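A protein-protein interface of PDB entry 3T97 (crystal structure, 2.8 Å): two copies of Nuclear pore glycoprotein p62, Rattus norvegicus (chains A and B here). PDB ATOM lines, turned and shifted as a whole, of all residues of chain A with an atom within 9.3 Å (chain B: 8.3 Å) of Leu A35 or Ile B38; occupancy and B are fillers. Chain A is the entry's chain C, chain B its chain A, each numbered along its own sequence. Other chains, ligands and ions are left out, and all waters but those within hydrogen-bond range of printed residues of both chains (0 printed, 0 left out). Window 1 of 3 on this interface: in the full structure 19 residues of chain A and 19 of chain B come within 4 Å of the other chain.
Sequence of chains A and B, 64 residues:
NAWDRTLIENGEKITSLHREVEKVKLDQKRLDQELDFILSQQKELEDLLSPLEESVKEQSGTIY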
ATOM      1  N   GLN A  28     -23.542 -12.319  12.512  1.00  0.00           N
ATOM      2  CA  GLN A  28     -22.954 -11.738  11.311  1.00  0.00           C
ATOM      3  C   GLN A  28     -21.499 -11.360  11.564  1.00  0.00           C
ATOM      4  O   GLN A  28     -20.610 -11.675  10.774  1.00  0.00           O
ATOM      5  CB  GLN A  28     -23.761 -10.508  10.901  1.00  0.00           C
ATOM      6  CG  GLN A  28     -23.572 -10.088   9.473  1.00  0.00           C
ATOM      7  CD  GLN A  28     -23.726 -11.245   8.520  1.00  0.00           C
ATOM      8  OE1 GLN A  28     -24.631 -12.065   8.667  1.00  0.00           O
ATOM      9  NE2 GLN A  28     -22.846 -11.316   7.530  1.00  0.00           N
ATOM     10  N   LYS A  29     -21.272 -10.686  12.682  1.00  0.00           N
ATOM     11  CA  LYS A  29     -19.944 -10.260  13.095  1.00  0.00           C
ATOM     12  C   LYS A  29     -19.003 -11.470  13.088  1.00  0.00           C
ATOM     13  O   LYS A  29     -17.846 -11.379  12.679  1.00  0.00           O
ATOM     14  CB  LYS A  29     -20.042  -9.662  14.497  1.00  0.00           C
ATOM     15  CG  LYS A  29     -18.750  -9.112  15.031  1.00  0.00           C
ATOM     16  CD  LYS A  29     -18.886  -8.665  16.473  1.00  0.00           C
ATOM     17  CE  LYS A  29     -17.506  -8.297  17.036  1.00  0.00           C
ATOM     18  NZ  LYS A  29     -17.539  -7.863  18.464  1.00  0.00           N
ATOM     19  N   ARG A  30     -19.522 -12.604  13.545  1.00  0.00           N
ATOM     20  CA  ARG A  30     -18.777 -13.854  13.616  1.00  0.00           C
ATOM     21  C   ARG A  30     -18.528 -14.438  12.239  1.00  0.00           C
ATOM     22  O   ARG A  30     -17.552 -15.142  12.039  1.00  0.00           O
ATOM     23  CB  ARG A  30     -19.551 -14.865  14.473  1.00  0.00           C
ATOM     24  CG  ARG A  30     -19.403 -16.330  14.059  1.00  0.00           C
ATOM     25  CD  ARG A  30     -20.214 -17.237  14.978  1.00  0.00           C
ATOM     26  NE  ARG A  30     -20.255 -18.626  14.525  1.00  0.00           N
ATOM     27  CZ  ARG A  30     -20.780 -19.627  15.229  1.00  0.00           C
ATOM     28  NH1 ARG A  30     -21.309 -19.400  16.428  1.00  0.00           N
ATOM     29  NH2 ARG A  30     -20.791 -20.859  14.731  1.00  0.00           N
ATOM     30  N   LEU A  31     -19.427 -14.160  11.298  1.00  0.00           N
ATOM     31  CA  LEU A  31     -19.284 -14.667   9.944  1.00  0.00           C
ATOM     32  C   LEU A  31     -18.250 -13.843   9.246  1.00  0.00           C
ATOM     33  O   LEU A  31     -17.447 -14.376   8.489  1.00  0.00           O
ATOM     34  CB  LEU A  31     -20.592 -14.580   9.164  1.00  0.00           C
ATOM     35  CG  LEU A  31     -21.657 -15.655   9.379  1.00  0.00           C
ATOM     36  CD1 LEU A  31     -22.857 -15.302   8.516  1.00  0.00           C
ATOM     37  CD2 LEU A  31     -21.137 -17.044   9.030  1.00  0.00           C
ATOM     38  N   ASP A  32     -18.275 -12.536   9.494  1.00  0.00           N
ATOM     39  CA  ASP A  32     -17.311 -11.631   8.873  1.00  0.00           C
ATOM     40  C   ASP A  32     -15.902 -11.973   9.351  1.00  0.00           C
ATOM     41  O   ASP A  32     -14.937 -11.806   8.612  1.00  0.00           O
ATOM     42  CB  ASP A  32     -17.647 -10.168   9.193  1.00  0.00           C
ATOM     43  CG  ASP A  32     -16.737  -9.171   8.465  1.00  0.00           C
ATOM     44  OD1 ASP A  32     -15.907  -9.593   7.629  1.00  0.00           O
ATOM     45  OD2 ASP A  32     -16.863  -7.949   8.726  1.00  0.00           O
ATOM     46  N   GLN A  33     -15.781 -12.468  10.581  1.00  0.00           N
ATOM     47  CA  GLN A  33     -14.475 -12.836  11.135  1.00  0.00           C
ATOM     48  C   GLN A  33     -13.891 -14.068  10.465  1.00  0.00           C
ATOM     49  O   GLN A  33     -12.689 -14.148  10.258  1.00  0.00           O
ATOM     50  CB  GLN A  33     -14.596 -13.044  12.647  1.00  0.00           C
ATOM     51  CG  GLN A  33     -14.890 -11.740  13.399  1.00  0.00           C
ATOM     52  CD  GLN A  33     -15.101 -11.921  14.896  1.00  0.00           C
ATOM     53  OE1 GLN A  33     -14.297 -12.561  15.573  1.00  0.00           O
ATOM     54  NE2 GLN A  33     -16.179 -11.338  15.420  1.00  0.00           N
ATOM     55  N   GLU A  34     -14.748 -15.026  10.124  1.00  0.00           N
ATOM     56  CA  GLU A  34     -14.328 -16.253   9.450  1.00  0.00           C
ATOM     57  C   GLU A  34     -13.818 -15.870   8.072  1.00  0.00           C
ATOM     58  O   GLU A  34     -12.883 -16.467   7.547  1.00  0.00           O
ATOM     59  CB  GLU A  34     -15.516 -17.215   9.268  1.00  0.00           C
ATOM     60  CG  GLU A  34     -16.261 -17.600  10.525  1.00  0.00           C
ATOM     61  CD  GLU A  34     -15.554 -18.678  11.319  1.00  0.00           C
ATOM     62  OE1 GLU A  34     -15.438 -19.808  10.804  1.00  0.00           O
ATOM     63  OE2 GLU A  34     -15.111 -18.394  12.449  1.00  0.00           O
ATOM     64  N   LEU A  35     -14.462 -14.869   7.487  1.00  0.00           N
ATOM     65  CA  LEU A  35     -14.115 -14.387   6.155  1.00  0.00           C
ATOM     66  C   LEU A  35     -12.694 -13.829   6.028  1.00  0.00           C
ATOM     67  O   LEU A  35     -11.967 -14.183   5.101  1.00  0.00           O
ATOM     68  CB  LEU A  35     -15.103 -13.312   5.717  1.00  0.00           C
ATOM     69  CG  LEU A  35     -15.100 -13.097   4.209  1.00  0.00           C
ATOM     70  CD1 LEU A  35     -16.010 -14.143   3.577  1.00  0.00           C
ATOM     71  CD2 LEU A  35     -15.559 -11.687   3.871  1.00  0.00           C
ATOM     72  N   ASP A  36     -12.302 -12.957   6.953  1.00  0.00           N
ATOM     73  CA  ASP A  36     -10.975 -12.354   6.925  1.00  0.00           C
ATOM     74  C   ASP A  36      -9.853 -13.358   7.159  1.00  0.00           C
ATOM     75  O   ASP A  36      -8.812 -13.274   6.534  1.00  0.00           O
ATOM     76  CB  ASP A  36     -10.887 -11.226   7.956  1.00  0.00           C
ATOM     77  CG  ASP A  36     -12.086 -10.299   7.914  1.00  0.00           C
ATOM     78  OD1 ASP A  36     -12.567 -10.000   6.800  1.00  0.00           O
ATOM     79  OD2 ASP A  36     -12.537  -9.865   8.994  1.00  0.00           O
ATOM     80  N   PHE A  37     -10.066 -14.298   8.068  1.00  0.00           N
ATOM     81  CA  PHE A  37      -9.075 -15.329   8.376  1.00  0.00           C
ATOM     82  C   PHE A  37      -8.764 -16.157   7.124  1.00  0.00           C
ATOM     83  O   PHE A  37      -7.663 -16.688   6.975  1.00  0.00           O
ATOM     84  CB  PHE A  37      -9.598 -16.254   9.496  1.00  0.00           C
ATOM     85  CG  PHE A  37      -8.690 -17.428   9.798  1.00  0.00           C
ATOM     86  CD1 PHE A  37      -7.478 -17.248  10.470  1.00  0.00           C
ATOM     87  CD2 PHE A  37      -9.042 -18.717   9.385  1.00  0.00           C
ATOM     88  CE1 PHE A  37      -6.628 -18.332  10.727  1.00  0.00           C
ATOM     89  CE2 PHE A  37      -8.195 -19.813   9.638  1.00  0.00           C
ATOM     90  CZ  PHE A  37      -6.987 -19.617  10.310  1.00  0.00           C
ATOM     91  N   ILE A  38      -9.746 -16.271   6.232  1.00  0.00           N
ATOM     92  CA  ILE A  38      -9.571 -17.013   4.998  1.00  0.00           C
ATOM     93  C   ILE A  38      -8.791 -16.168   4.004  1.00  0.00           C
ATOM     94  O   ILE A  38      -7.792 -16.604   3.463  1.00  0.00           O
ATOM     95  CB  ILE A  38     -10.927 -17.400   4.378  1.00  0.00           C
ATOM     96  CG1 ILE A  38     -11.624 -18.451   5.239  1.00  0.00           C
ATOM     97  CG2 ILE A  38     -10.718 -17.937   2.967  1.00  0.00           C
ATOM     98  CD1 ILE A  38     -12.852 -19.043   4.591  1.00  0.00           C
ATOM     99  N   LEU A  39      -9.260 -14.948   3.774  1.00  0.00           N
ATOM    100  CA  LEU A  39      -8.609 -14.023   2.850  1.00  0.00           C
ATOM    101  C   LEU A  39      -7.175 -13.736   3.298  1.00  0.00           C
ATOM    102  O   LEU A  39      -6.335 -13.291   2.518  1.00  0.00           O
ATOM    103  CB  LEU A  39      -9.381 -12.705   2.784  1.00  0.00           C
ATOM    104  CG  LEU A  39     -10.818 -12.782   2.317  1.00  0.00           C
ATOM    105  CD1 LEU A  39     -11.503 -11.430   2.508  1.00  0.00           C
ATOM    106  CD2 LEU A  39     -10.837 -13.220   0.863  1.00  0.00           C
ATOM    107  N   SER A  40      -6.921 -13.999   4.576  1.00  0.00           N
ATOM    108  CA  SER A  40      -5.633 -13.769   5.205  1.00  0.00           C
ATOM    109  C   SER A  40      -4.664 -14.905   4.929  1.00  0.00           C
ATOM    110  O   SER A  40      -3.587 -14.696   4.380  1.00  0.00           O
ATOM    111  CB  SER A  40      -5.847 -13.610   6.703  1.00  0.00           C
ATOM    112  OG  SER A  40      -4.664 -13.247   7.365  1.00  0.00           O
ATOM    113  N   GLN A  41      -5.059 -16.112   5.313  1.00  0.00           N
ATOM    114  CA  GLN A  41      -4.231 -17.299   5.129  1.00  0.00           C
ATOM    115  C   GLN A  41      -4.118 -17.625   3.650  1.00  0.00           C
ATOM    116  O   GLN A  41      -3.245 -18.381   3.223  1.00  0.00           O
ATOM    117  CB  GLN A  41      -4.853 -18.477   5.879  1.00  0.00           C
ATOM    118  CG  GLN A  41      -4.045 -19.742   5.819  1.00  0.00           C
ATOM    119  CD  GLN A  41      -4.684 -20.863   6.618  1.00  0.00           C
ATOM    120  OE1 GLN A  41      -4.143 -21.985   6.679  1.00  0.00           O
ATOM    121  NE2 GLN A  41      -5.843 -20.579   7.226  1.00  0.00           N
ATOM    122  N   GLN A  42      -5.004 -17.026   2.871  1.00  0.00           N
ATOM    123  CA  GLN A  42      -5.016 -17.277   1.455  1.00  0.00           C
ATOM    124  C   GLN A  42      -4.126 -16.317   0.703  1.00  0.00           C
ATOM    125  O   GLN A  42      -3.586 -16.673  -0.336  1.00  0.00           O
ATOM    126  CB  GLN A  42      -6.448 -17.200   0.953  1.00  0.00           C
ATOM    127  CG  GLN A  42      -6.721 -18.076  -0.232  1.00  0.00           C
ATOM    128  CD  GLN A  42      -8.189 -18.357  -0.394  1.00  0.00           C
ATOM    129  OE1 GLN A  42      -8.745 -19.218   0.286  1.00  0.00           O
ATOM    130  NE2 GLN A  42      -8.833 -17.610  -1.292  1.00  0.00           N
ATOM    131  N   LYS A  43      -3.962 -15.099   1.203  1.00  0.00           N
ATOM    132  CA  LYS A  43      -3.086 -14.156   0.520  1.00  0.00           C
ATOM    133  C   LYS A  43      -1.678 -14.522   0.922  1.00  0.00           C
ATOM    134  O   LYS A  43      -0.711 -14.120   0.287  1.00  0.00           O
ATOM    135  CB  LYS A  43      -3.392 -12.707   0.909  1.00  0.00           C
ATOM    136  CG  LYS A  43      -3.434 -12.421   2.404  1.00  0.00           C
ATOM    137  CD  LYS A  43      -3.801 -10.947   2.685  1.00  0.00           C
ATOM    138  CE  LYS A  43      -3.951 -10.646   4.182  1.00  0.00           C
ATOM    139  NZ  LYS A  43      -4.401  -9.245   4.450  1.00  0.00           N
ATOM    140  N   ASP B  27     -24.331  -6.156   4.690  1.00  0.00           N
ATOM    141  CA  ASP B  27     -23.163  -6.924   5.059  1.00  0.00           C
ATOM    142  C   ASP B  27     -23.215  -8.299   4.461  1.00  0.00           C
ATOM    143  O   ASP B  27     -22.187  -8.850   4.097  1.00  0.00           O
ATOM    144  CB  ASP B  27     -23.049  -6.993   6.563  1.00  0.00           C
ATOM    145  CG  ASP B  27     -22.798  -5.636   7.160  1.00  0.00           C
ATOM    146  OD1 ASP B  27     -23.512  -4.693   6.769  1.00  0.00           O
ATOM    147  OD2 ASP B  27     -21.890  -5.510   8.006  1.00  0.00           O
ATOM    148  N   ARG B  30     -22.205  -7.848   0.862  1.00  0.00           N
ATOM    149  CA  ARG B  30     -20.755  -7.685   0.821  1.00  0.00           C
ATOM    150  C   ARG B  30     -20.047  -9.007   1.049  1.00  0.00           C
ATOM    151  O   ARG B  30     -19.083  -9.339   0.367  1.00  0.00           O
ATOM    152  CB  ARG B  30     -20.287  -6.724   1.910  1.00  0.00           C
ATOM    153  CG  ARG B  30     -18.793  -6.830   2.216  1.00  0.00           C
ATOM    154  CD  ARG B  30     -18.343  -5.843   3.300  1.00  0.00           C
ATOM    155  NE  ARG B  30     -18.534  -6.311   4.676  1.00  0.00           N
ATOM    156  CZ  ARG B  30     -19.203  -5.635   5.617  1.00  0.00           C
ATOM    157  NH1 ARG B  30     -19.763  -4.457   5.329  1.00  0.00           N
ATOM    158  NH2 ARG B  30     -19.291  -6.123   6.851  1.00  0.00           N
ATOM    159  N   LEU B  31     -20.547  -9.745   2.034  1.00  0.00           N
ATOM    160  CA  LEU B  31     -20.006 -11.034   2.444  1.00  0.00           C
ATOM    161  C   LEU B  31     -20.049 -12.098   1.344  1.00  0.00           C
ATOM    162  O   LEU B  31     -19.147 -12.932   1.251  1.00  0.00           O
ATOM    163  CB  LEU B  31     -20.759 -11.519   3.688  1.00  0.00           C
ATOM    164  CG  LEU B  31     -20.071 -12.547   4.584  1.00  0.00           C
ATOM    165  CD1 LEU B  31     -18.673 -12.076   4.899  1.00  0.00           C
ATOM    166  CD2 LEU B  31     -20.860 -12.716   5.864  1.00  0.00           C
ATOM    167  N   ASP B  32     -21.101 -12.075   0.526  1.00  0.00           N
ATOM    168  CA  ASP B  32     -21.219 -13.024  -0.559  1.00  0.00           C
ATOM    169  C   ASP B  32     -20.278 -12.598  -1.669  1.00  0.00           C
ATOM    170  O   ASP B  32     -19.717 -13.425  -2.390  1.00  0.00           O
ATOM    171  CB  ASP B  32     -22.653 -13.082  -1.064  1.00  0.00           C
ATOM    172  CG  ASP B  32     -23.517 -13.964  -0.199  1.00  0.00           C
ATOM    173  OD1 ASP B  32     -23.290 -15.202  -0.206  1.00  0.00           O
ATOM    174  OD2 ASP B  32     -24.406 -13.427   0.504  1.00  0.00           O
ATOM    175  N   GLN B  33     -20.115 -11.292  -1.802  1.00  0.00           N
ATOM    176  CA  GLN B  33     -19.216 -10.748  -2.800  1.00  0.00           C
ATOM    177  C   GLN B  33     -17.820 -11.222  -2.482  1.00  0.00           C
ATOM    178  O   GLN B  33     -17.045 -11.498  -3.385  1.00  0.00           O
ATOM    179  CB  GLN B  33     -19.233  -9.229  -2.752  1.00  0.00           C
ATOM    180  CG  GLN B  33     -20.449  -8.590  -3.376  1.00  0.00           C
ATOM    181  CD  GLN B  33     -20.370  -7.102  -3.282  1.00  0.00           C
ATOM    182  OE1 GLN B  33     -20.939  -6.385  -4.103  1.00  0.00           O
ATOM    183  NE2 GLN B  33     -19.657  -6.611  -2.268  1.00  0.00           N
ATOM    184  N   GLU B  34     -17.498 -11.306  -1.191  1.00  0.00           N
ATOM    185  CA  GLU B  34     -16.176 -11.746  -0.769  1.00  0.00           C
ATOM    186  C   GLU B  34     -15.967 -13.231  -0.966  1.00  0.00           C
ATOM    187  O   GLU B  34     -14.826 -13.670  -1.164  1.00  0.00           O
ATOM    188  CB  GLU B  34     -15.908 -11.358   0.687  1.00  0.00           C
ATOM    189  CG  GLU B  34     -15.626  -9.879   0.902  1.00  0.00           C
ATOM    190  CD  GLU B  34     -14.636  -9.308  -0.118  1.00  0.00           C
ATOM    191  OE1 GLU B  34     -13.489  -9.787  -0.180  1.00  0.00           O
ATOM    192  OE2 GLU B  34     -15.013  -8.380  -0.871  1.00  0.00           O
ATOM    193  N   LEU B  35     -17.054 -14.007  -0.908  1.00  0.00           N
ATOM    194  CA  LEU B  35     -16.975 -15.455  -1.119  1.00  0.00           C
ATOM    195  C   LEU B  35     -16.626 -15.695  -2.580  1.00  0.00           C
ATOM    196  O   LEU B  35     -15.896 -16.617  -2.902  1.00  0.00           O
ATOM    197  CB  LEU B  35     -18.299 -16.140  -0.768  1.00  0.00           C
ATOM    198  CG  LEU B  35     -18.613 -16.316   0.715  1.00  0.00           C
ATOM    199  CD1 LEU B  35     -19.973 -16.948   0.905  1.00  0.00           C
ATOM    200  CD2 LEU B  35     -17.553 -17.187   1.334  1.00  0.00           C
ATOM    201  N   ASP B  36     -17.151 -14.848  -3.457  1.00  0.00           N
ATOM    202  CA  ASP B  36     -16.866 -14.953  -4.877  1.00  0.00           C
ATOM    203  C   ASP B  36     -15.380 -14.754  -5.130  1.00  0.00           C
ATOM    204  O   ASP B  36     -14.761 -15.480  -5.917  1.00  0.00           O
ATOM    205  CB  ASP B  36     -17.663 -13.924  -5.678  1.00  0.00           C
ATOM    206  CG  ASP B  36     -19.138 -14.250  -5.729  1.00  0.00           C
ATOM    207  OD1 ASP B  36     -19.465 -15.454  -5.687  1.00  0.00           O
ATOM    208  OD2 ASP B  36     -19.964 -13.311  -5.826  1.00  0.00           O
ATOM    209  N   PHE B  37     -14.809 -13.758  -4.467  1.00  0.00           N
ATOM    210  CA  PHE B  37     -13.383 -13.473  -4.578  1.00  0.00           C
ATOM    211  C   PHE B  37     -12.597 -14.697  -4.058  1.00  0.00           C
ATOM    212  O   PHE B  37     -11.779 -15.274  -4.772  1.00  0.00           O
ATOM    213  CB  PHE B  37     -13.025 -12.228  -3.757  1.00  0.00           C
ATOM    214  CG  PHE B  37     -11.592 -11.828  -3.886  1.00  0.00           C
ATOM    215  CD1 PHE B  37     -11.092 -11.412  -5.110  1.00  0.00           C
ATOM    216  CD2 PHE B  37     -10.725 -11.928  -2.805  1.00  0.00           C
ATOM    217  CE1 PHE B  37      -9.747 -11.105  -5.259  1.00  0.00           C
ATOM    218  CE2 PHE B  37      -9.379 -11.621  -2.948  1.00  0.00           C
ATOM    219  CZ  PHE B  37      -8.892 -11.211  -4.178  1.00  0.00           C
ATOM    220  N   ILE B  38     -12.857 -15.082  -2.809  1.00  0.00           N
ATOM    221  CA  ILE B  38     -12.230 -16.263  -2.219  1.00  0.00           C
ATOM    222  C   ILE B  38     -12.267 -17.429  -3.204  1.00  0.00           C
ATOM    223  O   ILE B  38     -11.269 -18.120  -3.399  1.00  0.00           O
ATOM    224  CB  ILE B  38     -12.976 -16.681  -0.942  1.00  0.00           C
ATOM    225  CG1 ILE B  38     -12.730 -15.641   0.156  1.00  0.00           C
ATOM    226  CG2 ILE B  38     -12.547 -18.065  -0.510  1.00  0.00           C
ATOM    227  CD1 ILE B  38     -13.509 -15.905   1.433  1.00  0.00           C
ATOM    228  N   LEU B  39     -13.428 -17.648  -3.815  1.00  0.00           N
ATOM    229  CA  LEU B  39     -13.597 -18.721  -4.772  1.00  0.00           C
ATOM    230  C   LEU B  39     -12.689 -18.601  -6.014  1.00  0.00           C
ATOM    231  O   LEU B  39     -11.999 -19.532  -6.387  1.00  0.00           O
ATOM    232  CB  LEU B  39     -15.049 -18.787  -5.218  1.00  0.00           C
ATOM    233  CG  LEU B  39     -15.255 -19.902  -6.257  1.00  0.00           C
ATOM    234  CD1 LEU B  39     -15.233 -21.245  -5.517  1.00  0.00           C
ATOM    235  CD2 LEU B  39     -16.549 -19.710  -7.020  1.00  0.00           C
ATOM    236  N   SER B  40     -12.699 -17.451  -6.666  1.00  0.00           N
ATOM    237  CA  SER B  40     -11.858 -17.276  -7.847  1.00  0.00           C
ATOM    238  C   SER B  40     -10.402 -17.252  -7.433  1.00  0.00           C
ATOM    239  O   SER B  40      -9.515 -17.314  -8.287  1.00  0.00           O
ATOM    240  CB  SER B  40     -12.187 -15.978  -8.578  1.00  0.00           C
ATOM    241  OG  SER B  40     -11.848 -14.863  -7.767  1.00  0.00           O
ATOM    242  N   GLN B  41     -10.156 -17.157  -6.126  1.00  0.00           N
ATOM    243  CA  GLN B  41      -8.792 -17.154  -5.640  1.00  0.00           C
ATOM    244  C   GLN B  41      -8.327 -18.575  -5.384  1.00  0.00           C
ATOM    245  O   GLN B  41      -7.196 -18.924  -5.707  1.00  0.00           O
ATOM    246  CB  GLN B  41      -8.646 -16.299  -4.378  1.00  0.00           C
ATOM    247  CG  GLN B  41      -7.178 -16.143  -3.934  1.00  0.00           C
ATOM    248  CD  GLN B  41      -6.953 -15.092  -2.872  1.00  0.00           C
ATOM    249  OE1 GLN B  41      -7.567 -15.114  -1.808  1.00  0.00           O
ATOM    250  NE2 GLN B  41      -6.047 -14.172  -3.153  1.00  0.00           N
ATOM    251  N   GLN B  42      -9.188 -19.406  -4.816  1.00  0.00           N
ATOM    252  CA  GLN B  42      -8.776 -20.783  -4.579  1.00  0.00           C
ATOM    253  C   GLN B  42      -8.483 -21.492  -5.895  1.00  0.00           C
ATOM    254  O   GLN B  42      -7.667 -22.421  -5.938  1.00  0.00           O
ATOM    255  CB  GLN B  42      -9.842 -21.560  -3.823  1.00  0.00           C
ATOM    256  CG  GLN B  42     -10.175 -20.985  -2.496  1.00  0.00           C
ATOM    257  CD  GLN B  42     -10.880 -21.993  -1.636  1.00  0.00           C
ATOM    258  OE1 GLN B  42     -11.706 -22.770  -2.122  1.00  0.00           O
ATOM    259  NE2 GLN B  42     -10.564 -21.995  -0.346  1.00  0.00           N
ATOM    260  N   LYS B  43      -9.159 -21.075  -6.963  1.00  0.00           N
ATOM    261  CA  LYS B  43      -8.936 -21.673  -8.273  1.00  0.00           C
ATOM    262  C   LYS B  43      -7.534 -21.302  -8.734  1.00  0.00           C
ATOM    263  O   LYS B  43      -6.721 -22.175  -9.006  1.00  0.00           O
ATOM    264  CB  LYS B  43      -9.969 -21.167  -9.273  1.00  0.00           C
ATOM    265  CG  LYS B  43     -11.335 -21.777  -9.056  1.00  0.00           C
ATOM    266  CD  LYS B  43     -12.443 -20.980  -9.708  1.00  0.00           C
ATOM    267  CE  LYS B  43     -13.800 -21.541  -9.329  1.00  0.00           C
ATOM    268  NZ  LYS B  43     -14.883 -20.518  -9.443  1.00  0.00           N
ATOM    269  N   GLU B  44      -7.245 -20.009  -8.805  1.00  0.00           N
ATOM    270  CA  GLU B  44      -5.928 -19.578  -9.224  1.00  0.00           C
ATOM    271  C   GLU B  44      -4.834 -20.188  -8.365  1.00  0.00           C
ATOM    272  O   GLU B  44      -3.721 -20.378  -8.821  1.00  0.00           O
ATOM    273  CB  GLU B  44      -5.835 -18.053  -9.195  1.00  0.00           C
ATOM    274  CG  GLU B  44      -6.743 -17.394 -10.229  1.00  0.00           C
ATOM    275  CD  GLU B  44      -6.448 -15.916 -10.447  1.00  0.00           C
ATOM    276  OE1 GLU B  44      -6.588 -15.132  -9.488  1.00  0.00           O
ATOM    277  OE2 GLU B  44      -6.081 -15.542 -11.583  1.00  0.00           O
ATOM    278  N   LEU B  45      -5.137 -20.500  -7.118  1.00  0.00           N
ATOM    279  CA  LEU B  45      -4.131 -21.102  -6.238  1.00  0.00           C
ATOM    280  C   LEU B  45      -3.903 -22.550  -6.654  1.00  0.00           C
ATOM    281  O   LEU B  45      -2.788 -23.034  -6.622  1.00  0.00           O
ATOM    282  CB  LEU B  45      -4.589 -21.045  -4.777  1.00  0.00           C
ATOM    283  CG  LEU B  45      -3.776 -20.195  -3.805  1.00  0.00           C
ATOM    284  CD1 LEU B  45      -3.375 -18.885  -4.465  1.00  0.00           C
ATOM    285  CD2 LEU B  45      -4.604 -19.941  -2.546  1.00  0.00           C
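The side-chain amide oxygen (OE1) of Gln A42 lies within hydrogen-bond range of the side-chain amide nitrogen (NE2) of Gln B42 (3.4 Å). The side-chain amide nitrogen of Gln A42 lies within hydrogen-bond range of the backbone carbonyl oxygen of Ile B38 (3.3 Å). NH2 of Arg B30 lies within salt-bridge range of OD2 of Asp A32 (3.6 Å). NE2 of Gln A42 is in hydrogen-bond range of OE1 of Gln B41, at 2.8 Å.
OD2 of Asp B27 is in salt-bridge range of NH2 of Arg B30. The side-chain hydroxyl (OG) of Ser B40 sits at hydrogen-bond distance from the backbone carbonyl oxygen (O) of Phe B37, at 3.0 Å.
Among the printed residues, merely in contact across the chains: Gln A28 with Leu B31, Leu A39 with Ile B38, Leu A35 with Glu B34, Leu A35 with Leu B31, Gln A42 with Leu B45, Leu A39 with Glu B34, Leu A35 with Ile B38, Ile A38 with Ile B38, Leu A31 with Leu B31 and Leu A39 with Phe B37.
Printed residues of chain B within 4 Å of Leu A35: Leu B31 (3.3 Å), Glu B34 (3.2 Å) and Ile B38 (3.7 Å). Ile B38 touches four residues of chain A. Printed residues of chain B within 4 Å of Ile A38: Ile B38 (3.8 Å). Of the printed residues of chain A, Leu B45 touches Gln A42. Asp A36 touches none of the printed residues of chain B. The nearest printed residue of chain B that does not touch Leu A39 is Gln B41 (4.6 Å).
Of the 16 printed residues of chain A, 7 touch a printed residue of chain B. Printed residues of chain A that touch a printed residue of chain B: Gln A28, Leu A31, Asp A32, Leu A35, Ile A38, Leu A39 and Gln A42. Hydrophobic or aromatic side chains of chain A within 4 Å of the printed part of chain B: Leu A31, Leu A35, Ile A38 and Leu A39. Of the 17 printed residues of chain B, 8 touch a printed residue of chain A. Hydrophobic or aromatic side chains of chain B within 4 Å of the printed part of chain A: Leu B31, Phe B37, Ile B38 and Leu B45. Among the printed residues, Asp or Glu carboxylates within 4 Å of a Lys or Arg side-chain nitrogen of the other chain: Asp A32 with Arg B30.
Leu A31 touches its own counterpart, Leu B31. Asp A32 touches Arg B30, but with the chains exchanged Arg A30 does not touch Asp B32 (12.2 Å). Leu A39 touches Glu B34, but with the chains exchanged Glu A34 does not touch Leu B39 (11.4 Å). Gln A42 touches Ile B38, but with the chains exchanged Ile A38 does not touch Gln B42 (5.2 Å). Positions printed for both chains: 30, 31, 32, 33, 34, 35, 36, 37, 38, 39, 40, 41, 42 and 43. Of the 14 pairs that touch across the chains among the printed residues, 3 have their exchanged pair printed and touching as well.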
